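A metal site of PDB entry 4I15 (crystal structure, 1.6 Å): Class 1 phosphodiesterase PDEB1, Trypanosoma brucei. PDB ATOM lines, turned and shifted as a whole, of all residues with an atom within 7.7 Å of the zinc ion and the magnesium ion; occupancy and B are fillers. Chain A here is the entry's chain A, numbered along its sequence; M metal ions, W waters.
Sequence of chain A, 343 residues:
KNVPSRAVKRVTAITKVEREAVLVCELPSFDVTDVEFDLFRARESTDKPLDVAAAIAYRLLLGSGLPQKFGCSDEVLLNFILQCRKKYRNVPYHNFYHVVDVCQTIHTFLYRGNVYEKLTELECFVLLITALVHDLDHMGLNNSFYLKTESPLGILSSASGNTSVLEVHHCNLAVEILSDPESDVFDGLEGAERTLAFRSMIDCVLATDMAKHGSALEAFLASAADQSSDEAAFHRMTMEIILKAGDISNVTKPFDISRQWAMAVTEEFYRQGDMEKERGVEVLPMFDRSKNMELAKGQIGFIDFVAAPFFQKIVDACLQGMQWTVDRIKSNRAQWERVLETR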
ATOM      1  N   TYR A  88     -37.190 -12.741  18.405  1.00  0.00           N
ATOM      2  CA  TYR A  88     -36.396 -12.943  19.609  1.00  0.00           C
ATOM      3  C   TYR A  88     -37.175 -12.419  20.793  1.00  0.00           C
ATOM      4  O   TYR A  88     -37.875 -11.421  20.694  1.00  0.00           O
ATOM      5  CB  TYR A  88     -35.024 -12.278  19.494  1.00  0.00           C
ATOM      6  CG  TYR A  88     -34.109 -13.054  18.585  1.00  0.00           C
ATOM      7  CD1 TYR A  88     -34.005 -12.737  17.229  1.00  0.00           C
ATOM      8  CD2 TYR A  88     -33.422 -14.173  19.056  1.00  0.00           C
ATOM      9  CE1 TYR A  88     -33.249 -13.533  16.355  1.00  0.00           C
ATOM     10  CE2 TYR A  88     -32.673 -14.970  18.197  1.00  0.00           C
ATOM     11  CZ  TYR A  88     -32.587 -14.647  16.853  1.00  0.00           C
ATOM     12  OH  TYR A  88     -31.879 -15.451  15.994  1.00  0.00           O
ATOM     13  N   TYR A  93     -30.130 -13.555  28.092  1.00  0.00           N
ATOM     14  CA  TYR A  93     -29.005 -13.770  27.190  1.00  0.00           C
ATOM     15  C   TYR A  93     -29.370 -14.083  25.743  1.00  0.00           C
ATOM     16  O   TYR A  93     -28.916 -13.397  24.823  1.00  0.00           O
ATOM     17  CB  TYR A  93     -28.133 -14.899  27.737  1.00  0.00           C
ATOM     18  CG  TYR A  93     -26.882 -15.154  26.921  1.00  0.00           C
ATOM     19  CD1 TYR A  93     -25.788 -14.287  27.008  1.00  0.00           C
ATOM     20  CD2 TYR A  93     -26.782 -16.266  26.087  1.00  0.00           C
ATOM     21  CE1 TYR A  93     -24.631 -14.528  26.271  1.00  0.00           C
ATOM     22  CE2 TYR A  93     -25.630 -16.514  25.353  1.00  0.00           C
ATOM     23  CZ  TYR A  93     -24.555 -15.642  25.452  1.00  0.00           C
ATOM     24  OH  TYR A  93     -23.405 -15.906  24.741  1.00  0.00           O
ATOM     25  N   HIS A  94     -30.185 -15.105  25.527  1.00  0.00           N
ATOM     26  CA  HIS A  94     -30.545 -15.468  24.168  1.00  0.00           C
ATOM     27  C   HIS A  94     -31.599 -14.568  23.526  1.00  0.00           C
ATOM     28  O   HIS A  94     -32.675 -15.034  23.130  1.00  0.00           O
ATOM     29  CB  HIS A  94     -30.969 -16.936  24.097  1.00  0.00           C
ATOM     30  CG  HIS A  94     -29.846 -17.897  24.333  1.00  0.00           C
ATOM     31  ND1 HIS A  94     -29.613 -18.490  25.551  1.00  0.00           N
ATOM     32  CD2 HIS A  94     -28.866 -18.339  23.513  1.00  0.00           C
ATOM     33  CE1 HIS A  94     -28.535 -19.243  25.479  1.00  0.00           C
ATOM     34  NE2 HIS A  94     -28.063 -19.171  24.250  1.00  0.00           N
ATOM     35  N   ASN A  95     -31.270 -13.287  23.442  1.00  0.00           N
ATOM     36  CA  ASN A  95     -32.130 -12.294  22.820  1.00  0.00           C
ATOM     37  C   ASN A  95     -31.482 -11.797  21.527  1.00  0.00           C
ATOM     38  O   ASN A  95     -30.464 -12.333  21.109  1.00  0.00           O
ATOM     39  CB  ASN A  95     -32.356 -11.122  23.779  1.00  0.00           C
ATOM     40  CG  ASN A  95     -31.071 -10.596  24.369  1.00  0.00           C
ATOM     41  OD1 ASN A  95     -30.121 -10.295  23.653  1.00  0.00           O
ATOM     42  ND2 ASN A  95     -31.025 -10.492  25.700  1.00  0.00           N
ATOM     43  N   HIS A  98     -27.640 -11.033  21.388  1.00  0.00           N
ATOM     44  CA  HIS A  98     -26.705 -12.157  21.317  1.00  0.00           C
ATOM     45  C   HIS A  98     -26.443 -12.538  19.854  1.00  0.00           C
ATOM     46  O   HIS A  98     -25.303 -12.778  19.478  1.00  0.00           O
ATOM     47  CB  HIS A  98     -27.251 -13.377  22.069  1.00  0.00           C
ATOM     48  CG  HIS A  98     -26.581 -14.675  21.712  1.00  0.00           C
ATOM     49  ND1 HIS A  98     -25.259 -14.927  21.994  1.00  0.00           N
ATOM     50  CD2 HIS A  98     -27.056 -15.783  21.102  1.00  0.00           C
ATOM     51  CE1 HIS A  98     -24.943 -16.139  21.573  1.00  0.00           C
ATOM     52  NE2 HIS A  98     -26.019 -16.679  21.032  1.00  0.00           N
ATOM     53  N   VAL A  99     -27.499 -12.583  19.045  1.00  0.00           N
ATOM     54  CA  VAL A  99     -27.306 -12.963  17.647  1.00  0.00           C
ATOM     55  C   VAL A  99     -26.620 -11.870  16.827  1.00  0.00           C
ATOM     56  O   VAL A  99     -25.869 -12.172  15.895  1.00  0.00           O
ATOM     57  CB  VAL A  99     -28.632 -13.420  16.981  1.00  0.00           C
ATOM     58  CG1 VAL A  99     -29.235 -14.560  17.784  1.00  0.00           C
ATOM     59  CG2 VAL A  99     -29.618 -12.263  16.899  1.00  0.00           C
ATOM     60  N   VAL A 102     -23.121 -12.290  17.636  1.00  0.00           N
ATOM     61  CA  VAL A 102     -22.544 -13.427  16.926  1.00  0.00           C
ATOM     62  C   VAL A 102     -22.237 -13.036  15.490  1.00  0.00           C
ATOM     63  O   VAL A 102     -21.193 -13.392  14.941  1.00  0.00           O
ATOM     64  CB  VAL A 102     -23.481 -14.650  17.001  1.00  0.00           C
ATOM     65  CG1 VAL A 102     -22.985 -15.772  16.072  1.00  0.00           C
ATOM     66  CG2 VAL A 102     -23.532 -15.165  18.440  1.00  0.00           C
ATOM     67  N   ALA A 131     -25.967 -16.236  11.403  1.00  0.00           N
ATOM     68  CA  ALA A 131     -25.765 -15.770  12.771  1.00  0.00           C
ATOM     69  C   ALA A 131     -27.059 -15.162  13.311  1.00  0.00           C
ATOM     70  O   ALA A 131     -27.413 -15.374  14.461  1.00  0.00           O
ATOM     71  CB  ALA A 131     -24.656 -14.722  12.803  1.00  0.00           C
ATOM     72  N   HIS A 134     -29.796 -18.116  14.008  1.00  0.00           N
ATOM     73  CA  HIS A 134     -29.413 -19.278  14.796  1.00  0.00           C
ATOM     74  C   HIS A 134     -30.051 -19.547  16.169  1.00  0.00           C
ATOM     75  O   HIS A 134     -29.946 -20.669  16.670  1.00  0.00           O
ATOM     76  CB  HIS A 134     -27.884 -19.371  14.886  1.00  0.00           C
ATOM     77  CG  HIS A 134     -27.307 -18.776  16.121  1.00  0.00           C
ATOM     78  ND1 HIS A 134     -27.014 -17.434  16.249  1.00  0.00           N
ATOM     79  CD2 HIS A 134     -26.966 -19.337  17.302  1.00  0.00           C
ATOM     80  CE1 HIS A 134     -26.512 -17.200  17.447  1.00  0.00           C
ATOM     81  NE2 HIS A 134     -26.472 -18.349  18.113  1.00  0.00           N
ATOM     82  N   ASP A 135     -30.709 -18.558  16.754  1.00  0.00           N
ATOM     83  CA  ASP A 135     -31.354 -18.743  18.055  1.00  0.00           C
ATOM     84  C   ASP A 135     -32.817 -18.251  18.047  1.00  0.00           C
ATOM     85  O   ASP A 135     -33.386 -17.970  19.090  1.00  0.00           O
ATOM     86  CB  ASP A 135     -30.589 -18.010  19.177  1.00  0.00           C
ATOM     87  CG  ASP A 135     -29.468 -18.863  19.770  1.00  0.00           C
ATOM     88  OD1 ASP A 135     -29.681 -20.085  19.860  1.00  0.00           O
ATOM     89  OD2 ASP A 135     -28.397 -18.317  20.151  1.00  0.00           O
ATOM     90  N   LEU A 136     -33.415 -18.184  16.869  1.00  0.00           N
ATOM     91  CA  LEU A 136     -34.799 -17.710  16.743  1.00  0.00           C
ATOM     92  C   LEU A 136     -35.793 -18.289  17.746  1.00  0.00           C
ATOM     93  O   LEU A 136     -35.880 -19.496  17.925  1.00  0.00           O
ATOM     94  CB  LEU A 136     -35.310 -17.977  15.316  1.00  0.00           C
ATOM     95  CG  LEU A 136     -34.731 -17.111  14.194  1.00  0.00           C
ATOM     96  CD1 LEU A 136     -35.178 -17.653  12.850  1.00  0.00           C
ATOM     97  CD2 LEU A 136     -35.180 -15.656  14.384  1.00  0.00           C
ATOM     98  N   HIS A 138     -35.791 -18.313  20.945  1.00  0.00           N
ATOM     99  CA  HIS A 138     -35.233 -18.990  22.105  1.00  0.00           C
ATOM    100  C   HIS A 138     -36.053 -18.488  23.288  1.00  0.00           C
ATOM    101  O   HIS A 138     -36.418 -17.312  23.329  1.00  0.00           O
ATOM    102  CB  HIS A 138     -33.757 -18.609  22.293  1.00  0.00           C
ATOM    103  CG  HIS A 138     -32.993 -19.558  23.161  1.00  0.00           C
ATOM    104  ND1 HIS A 138     -33.260 -19.721  24.507  1.00  0.00           N
ATOM    105  CD2 HIS A 138     -31.979 -20.402  22.875  1.00  0.00           C
ATOM    106  CE1 HIS A 138     -32.432 -20.628  25.015  1.00  0.00           C
ATOM    107  NE2 HIS A 138     -31.648 -21.054  24.044  1.00  0.00           N
ATOM    108  N   ASN A 143     -32.074 -27.270  25.862  1.00  0.00           N
ATOM    109  CA  ASN A 143     -32.699 -28.519  25.402  1.00  0.00           C
ATOM    110  C   ASN A 143     -33.002 -29.462  26.553  1.00  0.00           C
ATOM    111  O   ASN A 143     -34.073 -30.076  26.598  1.00  0.00           O
ATOM    112  CB  ASN A 143     -31.811 -29.247  24.395  1.00  0.00           C
ATOM    113  CG  ASN A 143     -31.624 -28.466  23.115  1.00  0.00           C
ATOM    114  OD1 ASN A 143     -32.436 -27.607  22.782  1.00  0.00           O
ATOM    115  ND2 ASN A 143     -30.564 -28.778  22.373  1.00  0.00           N
ATOM    116  N   LEU A 166     -34.168 -27.186  20.495  1.00  0.00           N
ATOM    117  CA  LEU A 166     -34.176 -25.806  20.059  1.00  0.00           C
ATOM    118  C   LEU A 166     -33.605 -25.557  18.666  1.00  0.00           C
ATOM    119  O   LEU A 166     -34.161 -24.776  17.896  1.00  0.00           O
ATOM    120  CB  LEU A 166     -33.438 -24.930  21.078  1.00  0.00           C
ATOM    121  CG  LEU A 166     -34.163 -24.822  22.412  1.00  0.00           C
ATOM    122  CD1 LEU A 166     -33.296 -24.107  23.426  1.00  0.00           C
ATOM    123  CD2 LEU A 166     -35.484 -24.079  22.209  1.00  0.00           C
ATOM    124  N   GLU A 167     -32.497 -26.221  18.349  1.00  0.00           N
ATOM    125  CA  GLU A 167     -31.869 -26.007  17.049  1.00  0.00           C
ATOM    126  C   GLU A 167     -32.801 -26.327  15.879  1.00  0.00           C
ATOM    127  O   GLU A 167     -32.836 -25.580  14.903  1.00  0.00           O
ATOM    128  CB  GLU A 167     -30.574 -26.818  16.936  1.00  0.00           C
ATOM    129  CG  GLU A 167     -29.432 -26.334  17.865  1.00  0.00           C
ATOM    130  CD  GLU A 167     -29.625 -26.711  19.327  1.00  0.00           C
ATOM    131  OE1 GLU A 167     -30.425 -27.630  19.622  1.00  0.00           O
ATOM    132  OE2 GLU A 167     -28.936 -26.115  20.194  1.00  0.00           O
ATOM    133  N   HIS A 170     -35.258 -23.439  15.703  1.00  0.00           N
ATOM    134  CA  HIS A 170     -34.721 -22.227  15.073  1.00  0.00           C
ATOM    135  C   HIS A 170     -34.705 -22.367  13.551  1.00  0.00           C
ATOM    136  O   HIS A 170     -35.006 -21.416  12.840  1.00  0.00           O
ATOM    137  CB  HIS A 170     -33.291 -21.925  15.538  1.00  0.00           C
ATOM    138  CG  HIS A 170     -33.113 -21.915  17.029  1.00  0.00           C
ATOM    139  ND1 HIS A 170     -33.993 -21.297  17.883  1.00  0.00           N
ATOM    140  CD2 HIS A 170     -32.137 -22.451  17.811  1.00  0.00           C
ATOM    141  CE1 HIS A 170     -33.574 -21.436  19.127  1.00  0.00           C
ATOM    142  NE2 HIS A 170     -32.449 -22.136  19.112  1.00  0.00           N
ATOM    143  N   VAL A 205     -26.716 -24.153  11.958  1.00  0.00           N
ATOM    144  CA  VAL A 205     -27.574 -24.013  13.139  1.00  0.00           C
ATOM    145  C   VAL A 205     -27.625 -25.316  13.942  1.00  0.00           C
ATOM    146  O   VAL A 205     -27.512 -25.309  15.168  1.00  0.00           O
ATOM    147  CB  VAL A 205     -29.010 -23.577  12.751  1.00  0.00           C
ATOM    148  CG1 VAL A 205     -29.897 -23.507  14.002  1.00  0.00           C
ATOM    149  CG2 VAL A 205     -28.958 -22.213  12.068  1.00  0.00           C
ATOM    150  N   THR A 208     -24.791 -26.009  16.361  1.00  0.00           N
ATOM    151  CA  THR A 208     -24.618 -25.205  17.571  1.00  0.00           C
ATOM    152  C   THR A 208     -25.038 -25.947  18.851  1.00  0.00           C
ATOM    153  O   THR A 208     -24.814 -25.454  19.964  1.00  0.00           O
ATOM    154  CB  THR A 208     -25.375 -23.855  17.494  1.00  0.00           C
ATOM    155  OG1 THR A 208     -26.765 -24.080  17.231  1.00  0.00           O
ATOM    156  CG2 THR A 208     -24.785 -22.976  16.390  1.00  0.00           C
ATOM    157  N   ASP A 209     -25.649 -27.121  18.702  1.00  0.00           N
ATOM    158  CA  ASP A 209     -26.063 -27.917  19.860  1.00  0.00           C
ATOM    159  C   ASP A 209     -24.761 -28.341  20.538  1.00  0.00           C
ATOM    160  O   ASP A 209     -23.983 -29.088  19.957  1.00  0.00           O
ATOM    161  CB  ASP A 209     -26.827 -29.153  19.389  1.00  0.00           C
ATOM    162  CG  ASP A 209     -27.385 -29.986  20.536  1.00  0.00           C
ATOM    163  OD1 ASP A 209     -26.907 -29.847  21.683  1.00  0.00           O
ATOM    164  OD2 ASP A 209     -28.309 -30.787  20.283  1.00  0.00           O
ATOM    165  N   MET A 210     -24.524 -27.878  21.768  1.00  0.00           N
ATOM    166  CA  MET A 210     -23.293 -28.213  22.460  1.00  0.00           C
ATOM    167  C   MET A 210     -23.093 -29.694  22.764  1.00  0.00           C
ATOM    168  O   MET A 210     -21.991 -30.112  23.131  1.00  0.00           O
ATOM    169  CB  MET A 210     -23.144 -27.387  23.744  1.00  0.00           C
ATOM    170  CG  MET A 210     -22.745 -25.936  23.490  1.00  0.00           C
ATOM    171  SD  MET A 210     -21.182 -25.740  22.578  1.00  0.00           S
ATOM    172  CE  MET A 210     -19.999 -25.946  23.912  1.00  0.00           C
ATOM    173  N   LEU A 243     -19.498 -20.745  13.074  1.00  0.00           N
ATOM    174  CA  LEU A 243     -20.707 -20.326  13.783  1.00  0.00           C
ATOM    175  C   LEU A 243     -20.575 -20.754  15.236  1.00  0.00           C
ATOM    176  O   LEU A 243     -20.957 -20.013  16.153  1.00  0.00           O
ATOM    177  CB  LEU A 243     -21.973 -20.942  13.176  1.00  0.00           C
ATOM    178  CG  LEU A 243     -23.256 -20.613  13.946  1.00  0.00           C
ATOM    179  CD1 LEU A 243     -23.475 -19.111  14.015  1.00  0.00           C
ATOM    180  CD2 LEU A 243     -24.446 -21.294  13.266  1.00  0.00           C
ATOM    181  N   GLY A 246     -18.326 -18.332  16.980  1.00  0.00           N
ATOM    182  CA  GLY A 246     -18.998 -17.089  17.300  1.00  0.00           C
ATOM    183  C   GLY A 246     -19.918 -17.262  18.485  1.00  0.00           C
ATOM    184  O   GLY A 246     -20.020 -16.387  19.362  1.00  0.00           O
ATOM    185  N   ASP A 247     -20.581 -18.417  18.542  1.00  0.00           N
ATOM    186  CA  ASP A 247     -21.520 -18.711  19.626  1.00  0.00           C
ATOM    187  C   ASP A 247     -20.857 -18.800  21.009  1.00  0.00           C
ATOM    188  O   ASP A 247     -21.469 -18.423  22.002  1.00  0.00           O
ATOM    189  CB  ASP A 247     -22.277 -20.015  19.298  1.00  0.00           C
ATOM    190  CG  ASP A 247     -23.708 -20.048  19.852  1.00  0.00           C
ATOM    191  OD1 ASP A 247     -24.336 -18.974  20.077  1.00  0.00           O
ATOM    192  OD2 ASP A 247     -24.212 -21.174  20.028  1.00  0.00           O
ATOM    193  N   ILE A 248     -19.614 -19.264  21.079  1.00  0.00           N
ATOM    194  CA  ILE A 248     -18.934 -19.347  22.382  1.00  0.00           C
ATOM    195  C   ILE A 248     -17.761 -18.367  22.476  1.00  0.00           C
ATOM    196  O   ILE A 248     -16.793 -18.614  23.189  1.00  0.00           O
ATOM    197  CB  ILE A 248     -18.414 -20.787  22.662  1.00  0.00           C
ATOM    198  CG1 ILE A 248     -17.358 -21.191  21.625  1.00  0.00           C
ATOM    199  CG2 ILE A 248     -19.576 -21.773  22.643  1.00  0.00           C
ATOM    200  CD1 ILE A 248     -16.706 -22.530  21.916  1.00  0.00           C
HETATM  201 ZN    ZN M   1     -26.382 -18.711  20.270  1.00  0.00          ZN
HETATM  202 MG    MG M   2     -28.522 -21.817  20.359  1.00  0.00          MG
HETATM  203  O   HOH W   1     -28.342 -21.491  22.626  1.00  0.00           O
HETATM  204  O   HOH W   2     -30.373 -22.889  20.975  1.00  0.00           O
HETATM  205  O   HOH W   3     -26.563 -20.851  20.126  1.00  0.00           O
HETATM  206  O   HOH W   4     -28.689 -22.479  18.224  1.00  0.00           O
HETATM  207  O   HOH W   5     -25.998 -19.483  22.563  1.00  0.00           O
HETATM  208  O   HOH W   6     -27.477 -23.898  20.576  1.00  0.00           O
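Of the 24 residues printed, 4 come within 4 Å of the zinc ion.
OD2 of Asp 135 is bound to the zinc ion, at 2.1 Å.
The side-chain carboxylate (OD1) of Asp 247 is bound to the zinc ion (2.1 Å).
The zinc ion is bound by water W3, 2.2 Å away.
A ring nitrogen (NE2) of His 134 is bound to the zinc ion (2.2 Å).
NE2 of His 98 is bound to the zinc ion.
Water W5 binds the zinc ion (2.4 Å).
One residue has an atom within 4 Å of the magnesium ion: Asp 135.
OD1 of Asp 135 binds the magnesium ion (2.1 Å).
The magnesium ion is bound by water W3 (2.2 Å).
Water W2 binds the magnesium ion (2.2 Å).
Water W4 is bound to the magnesium ion (2.2 Å).
Water W1 binds the magnesium ion (2.3 Å).
The magnesium ion is bound by water W6.
Water W6 bridges the side-chain carboxylate of Glu 167 (2.7 Å) and the backbone carbonyl oxygen of Thr 208 (3.1 Å).
Water W4 bridges the side-chain hydroxyl of Thr 208 (2.7 Å) and the backbone carbonyl oxygen of His 134 (2.7 Å).
The side-chain hydroxyl (OH) of Tyr 88 lies within hydrogen-bond range of the backbone NH (N) of Asp 135, at 3.4 Å.
The backbone carbonyl oxygen of Ala 131 sits at hydrogen-bond distance from a ring nitrogen (ND1) of His 134, 2.8 Å away.
The side-chain hydroxyl (OH) of Tyr 93 sits at hydrogen-bond distance from a ring nitrogen (ND1) of His 98.
N of His 98 sits at hydrogen-bond distance from OD1 of Asn 95 (3.4 Å).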
